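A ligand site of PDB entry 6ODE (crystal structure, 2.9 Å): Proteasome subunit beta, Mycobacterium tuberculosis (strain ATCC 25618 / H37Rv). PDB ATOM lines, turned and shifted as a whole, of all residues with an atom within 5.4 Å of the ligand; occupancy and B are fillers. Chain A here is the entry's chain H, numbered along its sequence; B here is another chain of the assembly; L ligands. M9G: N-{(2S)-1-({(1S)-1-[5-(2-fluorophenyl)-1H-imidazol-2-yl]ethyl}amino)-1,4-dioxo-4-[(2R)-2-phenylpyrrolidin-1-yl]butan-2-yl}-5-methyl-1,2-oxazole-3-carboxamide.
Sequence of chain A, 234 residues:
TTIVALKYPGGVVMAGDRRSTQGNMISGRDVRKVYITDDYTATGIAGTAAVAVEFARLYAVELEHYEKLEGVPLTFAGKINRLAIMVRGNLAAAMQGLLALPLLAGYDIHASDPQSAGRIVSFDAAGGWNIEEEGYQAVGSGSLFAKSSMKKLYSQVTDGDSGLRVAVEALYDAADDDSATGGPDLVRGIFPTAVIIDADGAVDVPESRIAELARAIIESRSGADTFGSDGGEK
OH of Tyr 35 lies within hydrogen-bond range of O of Arg 32 (3.1 Å).
The side-chain hydroxyl (OG) of Ser 27 sits close to the backbone NH (N) of Thr 21, at 3.4 Å.
O of Ser 20 lies within hydrogen-bond range of N of Ser 27 (2.6 Å).
The backbone carbonyl oxygen (O) of Lys 33 lies within hydrogen-bond range of the backbone NH (N) of Ile 45 (3.2 Å).
NZ of Lys 33 sits at hydrogen-bond distance from O of Arg 19 (2.7 Å).
The side-chain carboxylate of Asp 124 of chain B sits close to the backbone NH of Ala 126 of chain B, at 3.2 Å.
The side-chain carboxylate (OD1) of Asp 124 of chain B is in hydrogen-bond range of the backbone NH (N) of Gly 128 of chain B, 2.5 Å away.
The side-chain hydroxyl (OG1) of Thr 1 sits at hydrogen-bond distance from the side-chain amino group (NZ) of Lys 33, 3.0 Å away.
Ser 27 touches the ligand (O to C34, 3.9 Å).
Val 31 touches the ligand.
Lys 33 touches the ligand (CG to C10, 3.5 Å).
Tyr 35 touches the ligand (OH to C09, 3.9 Å).
Ile 45 touches the ligand.
Thr 48 touches the ligand.
Ala 52 touches the ligand (CB to C10, 3.5 Å).
CD2 of Leu 98 touches C26 of the ligand (3.9 Å).
Ser 122 of chain B touches the ligand.
Phe 123 of chain B touches the ligand (N to C39, 3.6 Å).
Ala 125 of chain B touches the ligand (N to O24, 3.9 Å).
Gly 128 of chain B touches the ligand.
O of Trp 129 of chain B touches C37 of the ligand (3.5 Å).
CB of Asn 130 of chain B touches C34 of the ligand, at 3.5 Å.
21 residues have an atom within 4 Å of the ligand: Ser 20, Thr 21, Gln 22, Ser 27, Val 31, Lys 33, Tyr 35, Ile 45, Gly 47, Thr 48, Ala 49, Ala 52, Leu 98, Ser 122 of chain B, Phe 123 of chain B, Asp 124 of chain B, Ala 125 of chain B, Ala 126 of chain B, Gly 128 of chain B, Trp 129 of chain B and Asn 130 of chain B.
The nearest printed residue that does not touch the ligand is Arg 32 (4.05 Å).
N of Ala 49 sits at hydrogen-bond distance from O17 of the ligand (3.1 Å).
The backbone NH (N) of Ala 126 of chain B is in hydrogen-bond range of an oxygen (O24) of the ligand.
N15 of the ligand lies within hydrogen-bond range of O of Thr 21 (3.0 Å).
The side-chain hydroxyl of Ser 20 sits at hydrogen-bond distance from a nitrogen (N14) of the ligand (2.9 Å).
OE1 of Gln 22 sits close to O41 of the ligand (2.7 Å).
The backbone carbonyl oxygen (O) of Gly 47 lies within hydrogen-bond range of a nitrogen (N04) of the ligand (2.7 Å).
OD2 of Asp 124 of chain B is in hydrogen-bond range of N19 of the ligand.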
ATOM      1  N   THR A   1       7.153 -10.334 -17.271  1.00  0.00           N
ATOM      2  CA  THR A   1       7.435 -11.757 -17.117  1.00  0.00           C
ATOM      3  C   THR A   1       8.523 -11.990 -16.073  1.00  0.00           C
ATOM      4  O   THR A   1       9.562 -11.328 -16.098  1.00  0.00           O
ATOM      5  CB  THR A   1       7.888 -12.381 -18.454  1.00  0.00           C
ATOM      6  OG1 THR A   1       6.904 -12.127 -19.469  1.00  0.00           O
ATOM      7  CG2 THR A   1       8.063 -13.892 -18.305  1.00  0.00           C
ATOM      8  N   ARG A  19       1.064 -12.847 -16.635  1.00  0.00           N
ATOM      9  CA  ARG A  19       0.745 -11.649 -17.393  1.00  0.00           C
ATOM     10  C   ARG A  19       1.382 -11.665 -18.776  1.00  0.00           C
ATOM     11  O   ARG A  19       2.496 -12.174 -18.955  1.00  0.00           O
ATOM     12  CB  ARG A  19       1.200 -10.398 -16.627  1.00  0.00           C
ATOM     13  CG  ARG A  19       1.071  -9.097 -17.412  1.00  0.00           C
ATOM     14  CD  ARG A  19       1.105  -7.892 -16.510  1.00  0.00           C
ATOM     15  NE  ARG A  19      -0.037  -7.884 -15.599  1.00  0.00           N
ATOM     16  CZ  ARG A  19      -0.290  -6.903 -14.742  1.00  0.00           C
ATOM     17  NH1 ARG A  19       0.513  -5.856 -14.670  1.00  0.00           N
ATOM     18  NH2 ARG A  19      -1.354  -6.975 -13.953  1.00  0.00           N
ATOM     19  N   SER A  20       0.665 -11.124 -19.748  1.00  0.00           N
ATOM     20  CA  SER A  20       1.217 -10.800 -21.056  1.00  0.00           C
ATOM     21  C   SER A  20       0.921  -9.338 -21.352  1.00  0.00           C
ATOM     22  O   SER A  20      -0.226  -8.903 -21.242  1.00  0.00           O
ATOM     23  CB  SER A  20       0.617 -11.677 -22.152  1.00  0.00           C
ATOM     24  OG  SER A  20       0.911 -11.144 -23.430  1.00  0.00           O
ATOM     25  N   THR A  21       1.960  -8.583 -21.712  1.00  0.00           N
ATOM     26  CA  THR A  21       1.801  -7.187 -22.074  1.00  0.00           C
ATOM     27  C   THR A  21       2.197  -6.973 -23.524  1.00  0.00           C
ATOM     28  O   THR A  21       2.876  -7.807 -24.140  1.00  0.00           O
ATOM     29  CB  THR A  21       2.623  -6.260 -21.185  1.00  0.00           C
ATOM     30  OG1 THR A  21       3.996  -6.681 -21.183  1.00  0.00           O
ATOM     31  CG2 THR A  21       2.097  -6.255 -19.760  1.00  0.00           C
ATOM     32  N   GLN A  22       1.762  -5.850 -24.072  1.00  0.00           N
ATOM     33  CA  GLN A  22       2.260  -5.333 -25.344  1.00  0.00           C
ATOM     34  C   GLN A  22       2.477  -3.842 -25.113  1.00  0.00           C
ATOM     35  O   GLN A  22       1.510  -3.068 -25.111  1.00  0.00           O
ATOM     36  CB  GLN A  22       1.312  -5.633 -26.499  1.00  0.00           C
ATOM     37  CG  GLN A  22       2.030  -5.865 -27.821  1.00  0.00           C
ATOM     38  CD  GLN A  22       1.095  -6.321 -28.924  1.00  0.00           C
ATOM     39  OE1 GLN A  22      -0.049  -6.697 -28.664  1.00  0.00           O
ATOM     40  NE2 GLN A  22       1.576  -6.272 -30.166  1.00  0.00           N
ATOM     41  N   SER A  27      -2.179  -7.674 -22.344  1.00  0.00           N
ATOM     42  CA  SER A  27      -2.674  -8.518 -23.418  1.00  0.00           C
ATOM     43  C   SER A  27      -2.992  -9.941 -22.983  1.00  0.00           C
ATOM     44  O   SER A  27      -3.500 -10.723 -23.795  1.00  0.00           O
ATOM     45  CB  SER A  27      -1.659  -8.560 -24.576  1.00  0.00           C
ATOM     46  OG  SER A  27      -0.402  -9.042 -24.116  1.00  0.00           O
ATOM     47  N   GLY A  28      -2.693 -10.299 -21.736  1.00  0.00           N
ATOM     48  CA  GLY A  28      -2.973 -11.635 -21.252  1.00  0.00           C
ATOM     49  C   GLY A  28      -2.941 -11.656 -19.736  1.00  0.00           C
ATOM     50  O   GLY A  28      -2.163 -10.939 -19.110  1.00  0.00           O
ATOM     51  N   VAL A  31      -1.345 -16.503 -18.849  1.00  0.00           N
ATOM     52  CA  VAL A  31      -0.340 -17.148 -19.678  1.00  0.00           C
ATOM     53  C   VAL A  31       0.367 -18.221 -18.865  1.00  0.00           C
ATOM     54  O   VAL A  31       0.705 -18.032 -17.695  1.00  0.00           O
ATOM     55  CB  VAL A  31       0.651 -16.102 -20.216  1.00  0.00           C
ATOM     56  CG1 VAL A  31       1.737 -16.767 -21.037  1.00  0.00           C
ATOM     57  CG2 VAL A  31      -0.084 -15.059 -21.041  1.00  0.00           C
ATOM     58  N   ARG A  32       0.598 -19.369 -19.504  1.00  0.00           N
ATOM     59  CA  ARG A  32       1.325 -20.482 -18.897  1.00  0.00           C
ATOM     60  C   ARG A  32       2.750 -20.465 -19.453  1.00  0.00           C
ATOM     61  O   ARG A  32       2.971 -20.784 -20.631  1.00  0.00           O
ATOM     62  CB  ARG A  32       0.633 -21.807 -19.187  1.00  0.00           C
ATOM     63  CG  ARG A  32      -0.694 -21.946 -18.460  1.00  0.00           C
ATOM     64  CD  ARG A  32      -1.654 -22.880 -19.178  1.00  0.00           C
ATOM     65  NE  ARG A  32      -3.009 -22.338 -19.142  1.00  0.00           N
ATOM     66  CZ  ARG A  32      -3.824 -22.399 -18.107  1.00  0.00           C
ATOM     67  NH1 ARG A  32      -3.422 -22.993 -16.981  1.00  0.00           N
ATOM     68  NH2 ARG A  32      -5.037 -21.871 -18.175  1.00  0.00           N
ATOM     69  N   LYS A  33       3.708 -20.101 -18.611  1.00  0.00           N
ATOM     70  CA  LYS A  33       5.090 -19.912 -19.033  1.00  0.00           C
ATOM     71  C   LYS A  33       6.036 -20.974 -18.492  1.00  0.00           C
ATOM     72  O   LYS A  33       7.228 -20.944 -18.824  1.00  0.00           O
ATOM     73  CB  LYS A  33       5.579 -18.526 -18.610  1.00  0.00           C
ATOM     74  CG  LYS A  33       4.645 -17.395 -19.015  1.00  0.00           C
ATOM     75  CD  LYS A  33       5.146 -16.063 -18.510  1.00  0.00           C
ATOM     76  CE  LYS A  33       4.115 -14.970 -18.741  1.00  0.00           C
ATOM     77  NZ  LYS A  33       4.625 -13.646 -18.316  1.00  0.00           N
ATOM     78  N   TYR A  35       6.710 -25.035 -18.361  1.00  0.00           N
ATOM     79  CA  TYR A  35       6.346 -26.256 -19.066  1.00  0.00           C
ATOM     80  C   TYR A  35       7.117 -27.439 -18.517  1.00  0.00           C
ATOM     81  O   TYR A  35       8.313 -27.338 -18.238  1.00  0.00           O
ATOM     82  CB  TYR A  35       6.656 -26.149 -20.575  1.00  0.00           C
ATOM     83  CG  TYR A  35       5.996 -24.997 -21.291  1.00  0.00           C
ATOM     84  CD1 TYR A  35       4.736 -25.138 -21.855  1.00  0.00           C
ATOM     85  CD2 TYR A  35       6.648 -23.779 -21.433  1.00  0.00           C
ATOM     86  CE1 TYR A  35       4.133 -24.089 -22.525  1.00  0.00           C
ATOM     87  CE2 TYR A  35       6.058 -22.732 -22.106  1.00  0.00           C
ATOM     88  CZ  TYR A  35       4.800 -22.893 -22.649  1.00  0.00           C
ATOM     89  OH  TYR A  35       4.206 -21.835 -23.314  1.00  0.00           O
ATOM     90  N   ILE A  45      10.154 -19.783 -19.632  1.00  0.00           N
ATOM     91  CA  ILE A  45      10.673 -18.921 -20.690  1.00  0.00           C
ATOM     92  C   ILE A  45      10.172 -17.499 -20.490  1.00  0.00           C
ATOM     93  O   ILE A  45       9.095 -17.260 -19.933  1.00  0.00           O
ATOM     94  CB  ILE A  45      10.282 -19.460 -22.086  1.00  0.00           C
ATOM     95  CG1 ILE A  45      10.458 -20.970 -22.123  1.00  0.00           C
ATOM     96  CG2 ILE A  45      11.121 -18.814 -23.154  1.00  0.00           C
ATOM     97  CD1 ILE A  45      10.185 -21.595 -23.465  1.00  0.00           C
ATOM     98  N   ALA A  46      10.991 -16.538 -20.934  1.00  0.00           N
ATOM     99  CA  ALA A  46      10.650 -15.126 -20.891  1.00  0.00           C
ATOM    100  C   ALA A  46      10.960 -14.498 -22.245  1.00  0.00           C
ATOM    101  O   ALA A  46      11.979 -14.803 -22.856  1.00  0.00           O
ATOM    102  CB  ALA A  46      11.437 -14.393 -19.791  1.00  0.00           C
ATOM    103  N   GLY A  47      10.074 -13.627 -22.708  1.00  0.00           N
ATOM    104  CA  GLY A  47      10.301 -12.928 -23.957  1.00  0.00           C
ATOM    105  C   GLY A  47       9.090 -13.043 -24.860  1.00  0.00           C
ATOM    106  O   GLY A  47       7.975 -13.320 -24.404  1.00  0.00           O
ATOM    107  N   THR A  48       9.319 -12.810 -26.154  1.00  0.00           N
ATOM    108  CA  THR A  48       8.229 -12.841 -27.123  1.00  0.00           C
ATOM    109  C   THR A  48       7.586 -14.218 -27.171  1.00  0.00           C
ATOM    110  O   THR A  48       8.280 -15.242 -27.268  1.00  0.00           O
ATOM    111  CB  THR A  48       8.736 -12.440 -28.514  1.00  0.00           C
ATOM    112  OG1 THR A  48       9.990 -13.084 -28.770  1.00  0.00           O
ATOM    113  CG2 THR A  48       8.913 -10.930 -28.593  1.00  0.00           C
ATOM    114  N   ALA A  49       6.251 -14.235 -27.115  1.00  0.00           N
ATOM    115  CA  ALA A  49       5.517 -15.475 -26.845  1.00  0.00           C
ATOM    116  C   ALA A  49       5.746 -16.529 -27.924  1.00  0.00           C
ATOM    117  O   ALA A  49       5.907 -17.711 -27.611  1.00  0.00           O
ATOM    118  CB  ALA A  49       4.032 -15.181 -26.692  1.00  0.00           C
ATOM    119  N   ALA A  50       5.748 -16.116 -29.195  1.00  0.00           N
ATOM    120  CA  ALA A  50       5.906 -17.073 -30.289  1.00  0.00           C
ATOM    121  C   ALA A  50       7.192 -17.873 -30.130  1.00  0.00           C
ATOM    122  O   ALA A  50       7.190 -19.108 -30.240  1.00  0.00           O
ATOM    123  CB  ALA A  50       5.891 -16.342 -31.621  1.00  0.00           C
ATOM    124  N   ALA A  52       8.828 -18.336 -27.375  1.00  0.00           N
ATOM    125  CA  ALA A  52       8.737 -19.151 -26.166  1.00  0.00           C
ATOM    126  C   ALA A  52       8.024 -20.464 -26.433  1.00  0.00           C
ATOM    127  O   ALA A  52       8.521 -21.549 -26.107  1.00  0.00           O
ATOM    128  CB  ALA A  52       8.041 -18.363 -25.060  1.00  0.00           C
ATOM    129  N   VAL A  53       6.839 -20.392 -27.044  1.00  0.00           N
ATOM    130  CA  VAL A  53       6.071 -21.596 -27.349  1.00  0.00           C
ATOM    131  C   VAL A  53       6.867 -22.514 -28.270  1.00  0.00           C
ATOM    132  O   VAL A  53       6.970 -23.725 -28.030  1.00  0.00           O
ATOM    133  CB  VAL A  53       4.701 -21.237 -27.945  1.00  0.00           C
ATOM    134  CG1 VAL A  53       3.907 -22.491 -28.240  1.00  0.00           C
ATOM    135  CG2 VAL A  53       3.926 -20.333 -26.989  1.00  0.00           C
ATOM    136  N   LEU A  98      12.750 -10.676 -31.887  1.00  0.00           N
ATOM    137  CA  LEU A  98      12.069 -11.907 -31.487  1.00  0.00           C
ATOM    138  C   LEU A  98      12.933 -12.677 -30.478  1.00  0.00           C
ATOM    139  O   LEU A  98      13.351 -13.806 -30.696  1.00  0.00           O
ATOM    140  CB  LEU A  98      11.756 -12.752 -32.718  1.00  0.00           C
ATOM    141  CG  LEU A  98      10.912 -11.998 -33.759  1.00  0.00           C
ATOM    142  CD1 LEU A  98      10.494 -12.897 -34.909  1.00  0.00           C
ATOM    143  CD2 LEU A  98       9.697 -11.354 -33.109  1.00  0.00           C
ATOM    144  N   LEU B  91       5.138 -12.801 -41.667  1.00  0.00           N
ATOM    145  CA  LEU B  91       5.803 -11.786 -40.844  1.00  0.00           C
ATOM    146  C   LEU B  91       6.648 -10.801 -41.666  1.00  0.00           C
ATOM    147  O   LEU B  91       6.595  -9.591 -41.434  1.00  0.00           O
ATOM    148  CB  LEU B  91       6.673 -12.453 -39.773  1.00  0.00           C
ATOM    149  CG  LEU B  91       7.525 -11.494 -38.931  1.00  0.00           C
ATOM    150  CD1 LEU B  91       6.675 -10.403 -38.312  1.00  0.00           C
ATOM    151  CD2 LEU B  91       8.294 -12.257 -37.863  1.00  0.00           C
ATOM    152  N   SER B 122      -6.652 -15.682 -30.469  1.00  0.00           N
ATOM    153  CA  SER B 122      -6.118 -14.470 -31.082  1.00  0.00           C
ATOM    154  C   SER B 122      -4.648 -14.666 -31.418  1.00  0.00           C
ATOM    155  O   SER B 122      -3.963 -15.517 -30.825  1.00  0.00           O
ATOM    156  CB  SER B 122      -6.305 -13.247 -30.169  1.00  0.00           C
ATOM    157  OG  SER B 122      -5.920 -13.548 -28.838  1.00  0.00           O
ATOM    158  N   PHE B 123      -4.166 -13.871 -32.374  1.00  0.00           N
ATOM    159  CA  PHE B 123      -2.835 -14.056 -32.940  1.00  0.00           C
ATOM    160  C   PHE B 123      -2.116 -12.724 -33.043  1.00  0.00           C
ATOM    161  O   PHE B 123      -2.727 -11.647 -32.997  1.00  0.00           O
ATOM    162  CB  PHE B 123      -2.913 -14.716 -34.333  1.00  0.00           C
ATOM    163  CG  PHE B 123      -3.570 -16.068 -34.330  1.00  0.00           C
ATOM    164  CD1 PHE B 123      -4.947 -16.182 -34.341  1.00  0.00           C
ATOM    165  CD2 PHE B 123      -2.804 -17.212 -34.332  1.00  0.00           C
ATOM    166  CE1 PHE B 123      -5.554 -17.430 -34.336  1.00  0.00           C
ATOM    167  CE2 PHE B 123      -3.406 -18.459 -34.340  1.00  0.00           C
ATOM    168  CZ  PHE B 123      -4.778 -18.564 -34.334  1.00  0.00           C
ATOM    169  N   ASP B 124      -0.792 -12.792 -33.192  1.00  0.00           N
ATOM    170  CA  ASP B 124       0.038 -11.620 -33.421  1.00  0.00           C
ATOM    171  C   ASP B 124       0.869 -11.818 -34.689  1.00  0.00           C
ATOM    172  O   ASP B 124       0.859 -12.883 -35.310  1.00  0.00           O
ATOM    173  CB  ASP B 124       0.949 -11.316 -32.212  1.00  0.00           C
ATOM    174  CG  ASP B 124       1.972 -12.417 -31.917  1.00  0.00           C
ATOM    175  OD1 ASP B 124       2.209 -13.314 -32.764  1.00  0.00           O
ATOM    176  OD2 ASP B 124       2.550 -12.393 -30.817  1.00  0.00           O
ATOM    177  N   ALA B 125       1.607 -10.766 -35.063  1.00  0.00           N
ATOM    178  CA  ALA B 125       2.345 -10.797 -36.317  1.00  0.00           C
ATOM    179  C   ALA B 125       3.455 -11.838 -36.309  1.00  0.00           C
ATOM    180  O   ALA B 125       3.816 -12.360 -37.369  1.00  0.00           O
ATOM    181  CB  ALA B 125       2.917  -9.410 -36.612  1.00  0.00           C
ATOM    182  N   ALA B 126       3.997 -12.166 -35.138  1.00  0.00           N
ATOM    183  CA  ALA B 126       5.084 -13.122 -35.027  1.00  0.00           C
ATOM    184  C   ALA B 126       4.612 -14.570 -34.927  1.00  0.00           C
ATOM    185  O   ALA B 126       5.435 -15.468 -34.756  1.00  0.00           O
ATOM    186  CB  ALA B 126       5.956 -12.795 -33.806  1.00  0.00           C
ATOM    187  N   GLY B 128       2.558 -15.787 -32.557  1.00  0.00           N
ATOM    188  CA  GLY B 128       2.066 -16.122 -31.238  1.00  0.00           C
ATOM    189  C   GLY B 128       0.544 -16.137 -31.198  1.00  0.00           C
ATOM    190  O   GLY B 128      -0.130 -15.348 -31.867  1.00  0.00           O
ATOM    191  N   TRP B 129       0.010 -17.056 -30.396  1.00  0.00           N
ATOM    192  CA  TRP B 129      -1.436 -17.254 -30.309  1.00  0.00           C
ATOM    193  C   TRP B 129      -1.832 -17.456 -28.866  1.00  0.00           C
ATOM    194  O   TRP B 129      -1.038 -17.931 -28.042  1.00  0.00           O
ATOM    195  CB  TRP B 129      -1.901 -18.447 -31.149  1.00  0.00           C
ATOM    196  CG  TRP B 129      -1.137 -19.698 -30.876  1.00  0.00           C
ATOM    197  CD1 TRP B 129      -0.054 -20.168 -31.562  1.00  0.00           C
ATOM    198  CD2 TRP B 129      -1.382 -20.638 -29.825  1.00  0.00           C
ATOM    199  NE1 TRP B 129       0.379 -21.349 -31.018  1.00  0.00           N
ATOM    200  CE2 TRP B 129      -0.416 -21.661 -29.946  1.00  0.00           C
ATOM    201  CE3 TRP B 129      -2.329 -20.729 -28.806  1.00  0.00           C
ATOM    202  CZ2 TRP B 129      -0.372 -22.747 -29.081  1.00  0.00           C
ATOM    203  CZ3 TRP B 129      -2.285 -21.802 -27.948  1.00  0.00           C
ATOM    204  CH2 TRP B 129      -1.305 -22.802 -28.084  1.00  0.00           C
ATOM    205  N   ASN B 130      -3.083 -17.115 -28.551  1.00  0.00           N
ATOM    206  CA  ASN B 130      -3.597 -17.227 -27.199  1.00  0.00           C
ATOM    207  C   ASN B 130      -5.076 -17.596 -27.249  1.00  0.00           C
ATOM    208  O   ASN B 130      -5.858 -16.929 -27.941  1.00  0.00           O
ATOM    209  CB  ASN B 130      -3.388 -15.926 -26.419  1.00  0.00           C
ATOM    210  CG  ASN B 130      -3.965 -15.988 -25.016  1.00  0.00           C
ATOM    211  OD1 ASN B 130      -3.434 -16.669 -24.138  1.00  0.00           O
ATOM    212  ND2 ASN B 130      -5.049 -15.260 -24.794  1.00  0.00           N
HETATM  213  C27 M9G L   1       5.982  -8.809 -31.424  1.00  0.00           C
HETATM  214  C25 M9G L   1       5.895  -9.042 -32.784  1.00  0.00           C
HETATM  215  C26 M9G L   1       6.945  -8.660 -33.806  1.00  0.00           C
HETATM  216  O24 M9G L   1       4.731  -9.656 -33.013  1.00  0.00           O
HETATM  217  N23 M9G L   1       4.086  -9.814 -31.819  1.00  0.00           N
HETATM  218  C22 M9G L   1       4.827  -9.308 -30.857  1.00  0.00           C
HETATM  219  C20 M9G L   1       4.471  -9.301 -29.391  1.00  0.00           C
HETATM  220  O21 M9G L   1       5.162  -8.711 -28.594  1.00  0.00           O
HETATM  221  C38 M9G L   1      -1.450 -13.595 -29.347  1.00  0.00           C
HETATM  222  C32 M9G L   1      -0.454 -13.700 -27.219  1.00  0.00           C
HETATM  223  C36 M9G L   1       0.306 -15.373 -25.647  1.00  0.00           C
HETATM  224  C33 M9G L   1      -1.211 -13.101 -26.207  1.00  0.00           C
HETATM  225  C16 M9G L   1       3.986 -10.687 -26.716  1.00  0.00           C
HETATM  226  C18 M9G L   1       2.867 -10.054 -27.581  1.00  0.00           C
HETATM  227  C28 M9G L   1       1.596 -10.935 -27.367  1.00  0.00           C
HETATM  228  C29 M9G L   1       0.242 -10.472 -28.008  1.00  0.00           C
HETATM  229  C40 M9G L   1      -2.032 -11.251 -29.283  1.00  0.00           C
HETATM  230  C39 M9G L   1      -2.618 -12.453 -29.469  1.00  0.00           C
HETATM  231  C31 M9G L   1      -0.449 -13.090 -28.681  1.00  0.00           C
HETATM  232  C37 M9G L   1       0.306 -14.840 -26.931  1.00  0.00           C
HETATM  233  C35 M9G L   1      -0.465 -14.773 -24.633  1.00  0.00           C
HETATM  234  C34 M9G L   1      -1.218 -13.627 -24.925  1.00  0.00           C
HETATM  235  N30 M9G L   1      -0.690 -11.509 -28.614  1.00  0.00           N
HETATM  236  N19 M9G L   1       3.235 -10.042 -28.945  1.00  0.00           N
HETATM  237  O17 M9G L   1       4.700 -11.562 -27.160  1.00  0.00           O
HETATM  238  O41 M9G L   1      -0.044  -9.352 -28.009  1.00  0.00           O
HETATM  239  C10 M9G L   1       6.058 -18.044 -22.136  1.00  0.00           C
HETATM  240  C13 M9G L   1       3.281 -13.840 -23.499  1.00  0.00           C
HETATM  241  C01 M9G L   1       5.469  -9.957 -23.264  1.00  0.00           C
HETATM  242  C02 M9G L   1       5.191 -10.806 -24.469  1.00  0.00           C
HETATM  243  C03 M9G L   1       4.651 -12.239 -24.010  1.00  0.00           C
HETATM  244  C05 M9G L   1       4.616 -14.312 -23.379  1.00  0.00           C
HETATM  245  C06 M9G L   1       5.069 -15.589 -22.979  1.00  0.00           C
HETATM  246  C07 M9G L   1       4.365 -16.762 -23.283  1.00  0.00           C
HETATM  247  C09 M9G L   1       4.868 -17.986 -22.855  1.00  0.00           C
HETATM  248  C11 M9G L   1       6.762 -16.883 -21.826  1.00  0.00           C
HETATM  249  C12 M9G L   1       6.258 -15.659 -22.254  1.00  0.00           C
HETATM  250  F08 M9G L   1       3.191 -16.702 -23.996  1.00  0.00           F
HETATM  251  N04 M9G L   1       5.406 -13.293 -23.694  1.00  0.00           N
HETATM  252  N14 M9G L   1       3.356 -12.578 -23.885  1.00  0.00           N
HETATM  253  N15 M9G L   1       4.173 -10.208 -25.288  1.00  0.00           N
